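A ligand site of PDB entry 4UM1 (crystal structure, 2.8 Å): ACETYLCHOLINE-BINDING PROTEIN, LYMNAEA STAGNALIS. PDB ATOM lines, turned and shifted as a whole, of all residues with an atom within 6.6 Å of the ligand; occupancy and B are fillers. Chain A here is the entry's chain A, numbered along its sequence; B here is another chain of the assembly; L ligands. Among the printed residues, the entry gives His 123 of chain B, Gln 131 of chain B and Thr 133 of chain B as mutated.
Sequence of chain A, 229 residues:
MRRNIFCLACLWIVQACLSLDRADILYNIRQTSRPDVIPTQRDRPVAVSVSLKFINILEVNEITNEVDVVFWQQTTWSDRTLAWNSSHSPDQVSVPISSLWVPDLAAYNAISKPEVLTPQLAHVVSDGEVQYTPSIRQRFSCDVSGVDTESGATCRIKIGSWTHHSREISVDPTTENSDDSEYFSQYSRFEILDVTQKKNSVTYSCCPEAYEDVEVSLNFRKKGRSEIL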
ATOM      1  N   TYR A 108     -26.349  -9.318  16.137  1.00  0.00           N
ATOM      2  CA  TYR A 108     -25.845 -10.695  16.205  1.00  0.00           C
ATOM      3  C   TYR A 108     -24.578 -10.944  15.385  1.00  0.00           C
ATOM      4  O   TYR A 108     -23.761 -11.795  15.750  1.00  0.00           O
ATOM      5  CB  TYR A 108     -26.935 -11.686  15.793  1.00  0.00           C
ATOM      6  CG  TYR A 108     -27.938 -11.993  16.882  1.00  0.00           C
ATOM      7  CD1 TYR A 108     -28.872 -11.053  17.279  1.00  0.00           C
ATOM      8  CD2 TYR A 108     -27.934 -13.220  17.520  1.00  0.00           C
ATOM      9  CE1 TYR A 108     -29.788 -11.329  18.293  1.00  0.00           C
ATOM     10  CE2 TYR A 108     -28.844 -13.513  18.521  1.00  0.00           C
ATOM     11  CZ  TYR A 108     -29.771 -12.568  18.907  1.00  0.00           C
ATOM     12  OH  TYR A 108     -30.667 -12.865  19.905  1.00  0.00           O
ATOM     13  N   SER A 161     -33.473  -8.476  20.826  1.00  0.00           N
ATOM     14  CA  SER A 161     -33.220  -8.541  22.274  1.00  0.00           C
ATOM     15  C   SER A 161     -32.298  -9.719  22.649  1.00  0.00           C
ATOM     16  O   SER A 161     -32.456 -10.834  22.171  1.00  0.00           O
ATOM     17  CB  SER A 161     -34.511  -8.684  23.057  1.00  0.00           C
ATOM     18  OG  SER A 161     -34.210  -8.835  24.435  1.00  0.00           O
ATOM     19  N   TRP A 162     -31.356  -9.453  23.546  1.00  0.00           N
ATOM     20  CA  TRP A 162     -30.352 -10.458  23.892  1.00  0.00           C
ATOM     21  C   TRP A 162     -30.828 -11.423  24.952  1.00  0.00           C
ATOM     22  O   TRP A 162     -30.438 -12.590  24.932  1.00  0.00           O
ATOM     23  CB  TRP A 162     -29.044  -9.795  24.343  1.00  0.00           C
ATOM     24  CG  TRP A 162     -27.871 -10.749  24.355  1.00  0.00           C
ATOM     25  CD1 TRP A 162     -27.258 -11.271  25.448  1.00  0.00           C
ATOM     26  CD2 TRP A 162     -27.200 -11.291  23.214  1.00  0.00           C
ATOM     27  NE1 TRP A 162     -26.234 -12.105  25.057  1.00  0.00           N
ATOM     28  CE2 TRP A 162     -26.166 -12.127  23.688  1.00  0.00           C
ATOM     29  CE3 TRP A 162     -27.363 -11.149  21.822  1.00  0.00           C
ATOM     30  CZ2 TRP A 162     -25.306 -12.831  22.843  1.00  0.00           C
ATOM     31  CZ3 TRP A 162     -26.511 -11.851  20.972  1.00  0.00           C
ATOM     32  CH2 TRP A 162     -25.499 -12.683  21.481  1.00  0.00           C
ATOM     33  N   THR A 163     -31.642 -10.940  25.898  1.00  0.00           N
ATOM     34  CA  THR A 163     -32.090 -11.775  27.027  1.00  0.00           C
ATOM     35  C   THR A 163     -33.598 -11.915  27.195  1.00  0.00           C
ATOM     36  O   THR A 163     -34.046 -12.705  28.031  1.00  0.00           O
ATOM     37  CB  THR A 163     -31.523 -11.274  28.382  1.00  0.00           C
ATOM     38  OG1 THR A 163     -32.102  -9.993  28.699  1.00  0.00           O
ATOM     39  CG2 THR A 163     -30.022 -11.169  28.351  1.00  0.00           C
ATOM     40  N   HIS A 164     -34.382 -11.161  26.445  1.00  0.00           N
ATOM     41  CA  HIS A 164     -35.837 -11.224  26.597  1.00  0.00           C
ATOM     42  C   HIS A 164     -36.507 -11.944  25.428  1.00  0.00           C
ATOM     43  O   HIS A 164     -36.321 -11.562  24.272  1.00  0.00           O
ATOM     44  CB  HIS A 164     -36.417  -9.818  26.746  1.00  0.00           C
ATOM     45  CG  HIS A 164     -36.025  -9.139  28.029  1.00  0.00           C
ATOM     46  ND1 HIS A 164     -36.536  -9.511  29.251  1.00  0.00           N
ATOM     47  CD2 HIS A 164     -35.184  -8.100  28.260  1.00  0.00           C
ATOM     48  CE1 HIS A 164     -36.025  -8.738  30.190  1.00  0.00           C
ATOM     49  NE2 HIS A 164     -35.205  -7.866  29.624  1.00  0.00           N
ATOM     50  N   HIS A 165     -37.297 -12.967  25.719  1.00  0.00           N
ATOM     51  CA  HIS A 165     -38.004 -13.709  24.662  1.00  0.00           C
ATOM     52  C   HIS A 165     -39.245 -12.974  24.124  1.00  0.00           C
ATOM     53  O   HIS A 165     -39.553 -11.870  24.531  1.00  0.00           O
ATOM     54  CB  HIS A 165     -38.334 -15.150  25.100  1.00  0.00           C
ATOM     55  CG  HIS A 165     -39.219 -15.220  26.302  1.00  0.00           C
ATOM     56  ND1 HIS A 165     -40.516 -14.751  26.321  1.00  0.00           N
ATOM     57  CD2 HIS A 165     -38.997 -15.733  27.546  1.00  0.00           C
ATOM     58  CE1 HIS A 165     -41.056 -14.955  27.500  1.00  0.00           C
ATOM     59  NE2 HIS A 165     -40.157 -15.554  28.262  1.00  0.00           N
ATOM     60  N   TYR A 204     -33.695 -20.848  19.848  1.00  0.00           N
ATOM     61  CA  TYR A 204     -32.318 -21.294  20.064  1.00  0.00           C
ATOM     62  C   TYR A 204     -32.255 -22.607  20.875  1.00  0.00           C
ATOM     63  O   TYR A 204     -33.216 -22.989  21.550  1.00  0.00           O
ATOM     64  CB  TYR A 204     -31.482 -20.194  20.725  1.00  0.00           C
ATOM     65  CG  TYR A 204     -31.353 -18.966  19.878  1.00  0.00           C
ATOM     66  CD1 TYR A 204     -32.312 -17.956  19.930  1.00  0.00           C
ATOM     67  CD2 TYR A 204     -30.277 -18.800  19.008  1.00  0.00           C
ATOM     68  CE1 TYR A 204     -32.209 -16.821  19.147  1.00  0.00           C
ATOM     69  CE2 TYR A 204     -30.158 -17.659  18.219  1.00  0.00           C
ATOM     70  CZ  TYR A 204     -31.127 -16.665  18.285  1.00  0.00           C
ATOM     71  OH  TYR A 204     -31.023 -15.529  17.502  1.00  0.00           O
ATOM     72  N   CYS A 206     -30.835 -23.335  23.533  1.00  0.00           N
ATOM     73  CA  CYS A 206     -30.798 -23.202  24.976  1.00  0.00           C
ATOM     74  C   CYS A 206     -32.198 -23.267  25.623  1.00  0.00           C
ATOM     75  O   CYS A 206     -32.369 -23.930  26.640  1.00  0.00           O
ATOM     76  CB  CYS A 206     -30.084 -21.897  25.374  1.00  0.00           C
ATOM     77  SG  CYS A 206     -31.123 -20.371  25.273  1.00  0.00           S
ATOM     78  N   CYS A 207     -33.184 -22.613  25.009  1.00  0.00           N
ATOM     79  CA  CYS A 207     -34.500 -22.372  25.643  1.00  0.00           C
ATOM     80  C   CYS A 207     -35.675 -22.725  24.708  1.00  0.00           C
ATOM     81  O   CYS A 207     -35.526 -22.685  23.484  1.00  0.00           O
ATOM     82  CB  CYS A 207     -34.597 -20.900  26.109  1.00  0.00           C
ATOM     83  SG  CYS A 207     -32.992 -19.990  26.014  1.00  0.00           S
ATOM     84  N   TYR A 211     -37.232 -16.038  20.224  1.00  0.00           N
ATOM     85  CA  TYR A 211     -36.645 -14.698  20.320  1.00  0.00           C
ATOM     86  C   TYR A 211     -36.820 -13.946  19.020  1.00  0.00           C
ATOM     87  O   TYR A 211     -36.353 -14.390  17.990  1.00  0.00           O
ATOM     88  CB  TYR A 211     -35.157 -14.773  20.696  1.00  0.00           C
ATOM     89  CG  TYR A 211     -34.935 -15.213  22.120  1.00  0.00           C
ATOM     90  CD1 TYR A 211     -35.063 -16.549  22.480  1.00  0.00           C
ATOM     91  CD2 TYR A 211     -34.614 -14.295  23.118  1.00  0.00           C
ATOM     92  CE1 TYR A 211     -34.873 -16.969  23.788  1.00  0.00           C
ATOM     93  CE2 TYR A 211     -34.423 -14.700  24.445  1.00  0.00           C
ATOM     94  CZ  TYR A 211     -34.553 -16.045  24.771  1.00  0.00           C
ATOM     95  OH  TYR A 211     -34.370 -16.478  26.068  1.00  0.00           O
ATOM     96  N   TRP B  72     -19.698 -17.040  22.040  1.00  0.00           N
ATOM     97  CA  TRP B  72     -20.564 -16.877  23.210  1.00  0.00           C
ATOM     98  C   TRP B  72     -19.974 -17.709  24.329  1.00  0.00           C
ATOM     99  O   TRP B  72     -19.679 -18.883  24.120  1.00  0.00           O
ATOM    100  CB  TRP B  72     -21.984 -17.371  22.941  1.00  0.00           C
ATOM    101  CG  TRP B  72     -22.697 -16.649  21.886  1.00  0.00           C
ATOM    102  CD1 TRP B  72     -22.235 -15.600  21.142  1.00  0.00           C
ATOM    103  CD2 TRP B  72     -24.027 -16.912  21.417  1.00  0.00           C
ATOM    104  NE1 TRP B  72     -23.195 -15.195  20.244  1.00  0.00           N
ATOM    105  CE2 TRP B  72     -24.300 -15.979  20.391  1.00  0.00           C
ATOM    106  CE3 TRP B  72     -25.012 -17.838  21.785  1.00  0.00           C
ATOM    107  CZ2 TRP B  72     -25.534 -15.962  19.717  1.00  0.00           C
ATOM    108  CZ3 TRP B  72     -26.237 -17.822  21.117  1.00  0.00           C
ATOM    109  CH2 TRP B  72     -26.481 -16.889  20.083  1.00  0.00           C
ATOM    110  N   GLN B  92     -38.954 -15.819  35.985  1.00  0.00           N
ATOM    111  CA  GLN B  92     -37.650 -15.361  35.530  1.00  0.00           C
ATOM    112  C   GLN B  92     -37.559 -13.829  35.408  1.00  0.00           C
ATOM    113  O   GLN B  92     -38.558 -13.171  35.133  1.00  0.00           O
ATOM    114  CB  GLN B  92     -37.385 -15.954  34.160  1.00  0.00           C
ATOM    115  CG  GLN B  92     -38.495 -15.598  33.208  1.00  0.00           C
ATOM    116  CD  GLN B  92     -38.129 -15.931  31.793  1.00  0.00           C
ATOM    117  OE1 GLN B  92     -37.537 -16.976  31.528  1.00  0.00           O
ATOM    118  NE2 GLN B  92     -38.485 -15.041  30.874  1.00  0.00           N
ATOM    119  N   THR B 118     -22.041  -7.612  23.954  1.00  0.00           N
ATOM    120  CA  THR B 118     -23.473  -7.592  24.232  1.00  0.00           C
ATOM    121  C   THR B 118     -23.773  -6.865  25.546  1.00  0.00           C
ATOM    122  O   THR B 118     -22.840  -6.597  26.326  1.00  0.00           O
ATOM    123  CB  THR B 118     -23.990  -9.024  24.293  1.00  0.00           C
ATOM    124  OG1 THR B 118     -23.129  -9.791  25.145  1.00  0.00           O
ATOM    125  CG2 THR B 118     -24.034  -9.630  22.921  1.00  0.00           C
ATOM    126  N   LEU B 121     -26.287  -8.420  30.980  1.00  0.00           N
ATOM    127  CA  LEU B 121     -27.410  -8.899  31.802  1.00  0.00           C
ATOM    128  C   LEU B 121     -27.332 -10.396  31.982  1.00  0.00           C
ATOM    129  O   LEU B 121     -26.952 -11.128  31.066  1.00  0.00           O
ATOM    130  CB  LEU B 121     -28.753  -8.558  31.142  1.00  0.00           C
ATOM    131  CG  LEU B 121     -28.987  -7.065  30.908  1.00  0.00           C
ATOM    132  CD1 LEU B 121     -30.325  -6.800  30.211  1.00  0.00           C
ATOM    133  CD2 LEU B 121     -28.892  -6.347  32.236  1.00  0.00           C
ATOM    134  N   ALA B 122     -27.710 -10.869  33.166  1.00  0.00           N
ATOM    135  CA  ALA B 122     -27.859 -12.295  33.417  1.00  0.00           C
ATOM    136  C   ALA B 122     -29.345 -12.688  33.512  1.00  0.00           C
ATOM    137  O   ALA B 122     -30.220 -11.877  33.890  1.00  0.00           O
ATOM    138  CB  ALA B 122     -27.128 -12.689  34.660  1.00  0.00           C
ATOM    139  N   HIS B 123     -29.603 -13.946  33.188  1.00  0.00           N
ATOM    140  CA  HIS B 123     -30.947 -14.515  33.296  1.00  0.00           C
ATOM    141  C   HIS B 123     -31.044 -15.223  34.639  1.00  0.00           C
ATOM    142  O   HIS B 123     -30.168 -16.007  34.997  1.00  0.00           O
ATOM    143  CB  HIS B 123     -31.150 -15.494  32.159  1.00  0.00           C
ATOM    144  CG  HIS B 123     -32.584 -15.881  31.946  1.00  0.00           C
ATOM    145  ND1 HIS B 123     -33.069 -17.114  32.324  1.00  0.00           N
ATOM    146  CD2 HIS B 123     -33.595 -15.224  31.354  1.00  0.00           C
ATOM    147  CE1 HIS B 123     -34.348 -17.192  31.989  1.00  0.00           C
ATOM    148  NE2 HIS B 123     -34.693 -16.069  31.407  1.00  0.00           N
ATOM    149  N   GLN B 131     -27.916 -17.779  34.456  1.00  0.00           N
ATOM    150  CA  GLN B 131     -27.158 -17.983  33.228  1.00  0.00           C
ATOM    151  C   GLN B 131     -26.687 -16.650  32.661  1.00  0.00           C
ATOM    152  O   GLN B 131     -27.480 -15.738  32.456  1.00  0.00           O
ATOM    153  CB  GLN B 131     -27.979 -18.740  32.198  1.00  0.00           C
ATOM    154  CG  GLN B 131     -27.209 -18.993  30.924  1.00  0.00           C
ATOM    155  CD  GLN B 131     -28.013 -19.774  29.903  1.00  0.00           C
ATOM    156  OE1 GLN B 131     -28.754 -20.694  30.263  1.00  0.00           O
ATOM    157  NE2 GLN B 131     -27.853 -19.411  28.615  1.00  0.00           N
ATOM    158  N   TYR B 132     -25.397 -16.540  32.402  1.00  0.00           N
ATOM    159  CA  TYR B 132     -24.824 -15.341  31.806  1.00  0.00           C
ATOM    160  C   TYR B 132     -24.054 -15.739  30.547  1.00  0.00           C
ATOM    161  O   TYR B 132     -23.071 -16.475  30.610  1.00  0.00           O
ATOM    162  CB  TYR B 132     -23.906 -14.647  32.821  1.00  0.00           C
ATOM    163  CG  TYR B 132     -23.180 -13.417  32.288  1.00  0.00           C
ATOM    164  CD1 TYR B 132     -23.843 -12.474  31.525  1.00  0.00           C
ATOM    165  CD2 TYR B 132     -21.835 -13.193  32.597  1.00  0.00           C
ATOM    166  CE1 TYR B 132     -23.202 -11.354  31.053  1.00  0.00           C
ATOM    167  CE2 TYR B 132     -21.175 -12.087  32.130  1.00  0.00           C
ATOM    168  CZ  TYR B 132     -21.867 -11.167  31.335  1.00  0.00           C
ATOM    169  OH  TYR B 132     -21.231 -10.021  30.837  1.00  0.00           O
ATOM    170  N   THR B 133     -24.504 -15.244  29.400  1.00  0.00           N
ATOM    171  CA  THR B 133     -23.951 -15.629  28.094  1.00  0.00           C
ATOM    172  C   THR B 133     -23.543 -14.410  27.254  1.00  0.00           C
ATOM    173  O   THR B 133     -24.249 -13.997  26.329  1.00  0.00           O
ATOM    174  CB  THR B 133     -24.973 -16.492  27.292  1.00  0.00           C
ATOM    175  OG1 THR B 133     -25.591 -17.478  28.140  1.00  0.00           O
ATOM    176  CG2 THR B 133     -24.313 -17.166  26.091  1.00  0.00           C
ATOM    177  N   PRO B 134     -22.400 -13.802  27.582  1.00  0.00           N
ATOM    178  CA  PRO B 134     -21.979 -12.639  26.788  1.00  0.00           C
ATOM    179  C   PRO B 134     -21.303 -13.067  25.487  1.00  0.00           C
ATOM    180  O   PRO B 134     -20.663 -14.120  25.427  1.00  0.00           O
ATOM    181  CB  PRO B 134     -20.940 -11.968  27.686  1.00  0.00           C
ATOM    182  CG  PRO B 134     -20.379 -13.092  28.508  1.00  0.00           C
ATOM    183  CD  PRO B 134     -21.498 -14.056  28.727  1.00  0.00           C
HETATM  184  C1  LIG L   1     -28.268 -14.601  22.459  1.00  0.00           C
HETATM  185  N1  LIG L   1     -29.675 -14.122  22.447  1.00  0.00           N
HETATM  186  C2  LIG L   1     -30.778 -15.086  22.190  1.00  0.00           C
HETATM  187  C3  LIG L   1     -31.065 -15.993  23.410  1.00  0.00           C
HETATM  188  C4  LIG L   1     -29.838 -16.796  23.846  1.00  0.00           C
HETATM  189  N2  LIG L   1     -28.934 -15.900  24.577  1.00  0.00           N
HETATM  190  C5  LIG L   1     -27.837 -15.419  23.702  1.00  0.00           C
HETATM  191  C6  LIG L   1     -28.975 -15.430  28.747  1.00  0.00           C
HETATM  192  C7  LIG L   1     -29.856 -16.366  28.161  1.00  0.00           C
HETATM  193  C8  LIG L   1     -29.848 -16.516  26.739  1.00  0.00           C
HETATM  194  C9  LIG L   1     -28.961 -15.752  25.937  1.00  0.00           C
HETATM  195  C10 LIG L   1     -28.127 -14.859  26.665  1.00  0.00           C
HETATM  196  N3  LIG L   1     -28.132 -14.699  28.010  1.00  0.00           N
HETATM  197  O1  LIG L   1     -30.717 -17.038  29.011  1.00  0.00           O
HETATM  198  C11 LIG L   1     -32.090 -16.663  28.854  1.00  0.00           C
HETATM  199  C12 LIG L   1     -32.944 -17.918  28.911  1.00  0.00           C
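Tyr 204 touches the ligand.
Cys 207 touches the ligand.
Tyr 211 touches the ligand (OH to C12, 3.5 Å).
Trp 72 of chain B touches the ligand (CH2 to C1, 3.8 Å).
His 123 of chain B touches the ligand.
Gln 131 of chain B touches the ligand.
CB of Thr 133 of chain B touches C10 of the ligand, 3.6 Å away.
Hydrophobic or aromatic side chains within 4 Å of the ligand: Tyr 108, Trp 162, Tyr 204, Tyr 211, Trp 72 of chain B and His 123 of chain B.
N1 of the ligand lies within hydrogen-bond range of OH of Tyr 108, at 3.0 Å.
The backbone carbonyl oxygen (O) of Trp 162 sits at hydrogen-bond distance from a nitrogen (N1) of the ligand (3.0 Å).
O of Thr 133 of chain B is in hydrogen-bond range of NE1 of Trp 162, 3.0 Å away.
The backbone NH (N) of His 123 of chain B lies within hydrogen-bond range of the backbone carbonyl oxygen (O) of Gln 131 of chain B, at 2.9 Å.
OE1 of Gln 92 of chain B sits at hydrogen-bond distance from NE2 of His 123 of chain B (3.0 Å).
The side-chain hydroxyl of Tyr 211 sits at hydrogen-bond distance from the side-chain sulfur of Cys 207, 3.8 Å away.
The side-chain sulfur of Cys 206 forms a disulfide with the side-chain sulfur of Cys 207 (2.0 Å).
NE2 of Gln 131 of chain B is in hydrogen-bond range of OG1 of Thr 133 of chain B, at 3.0 Å.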
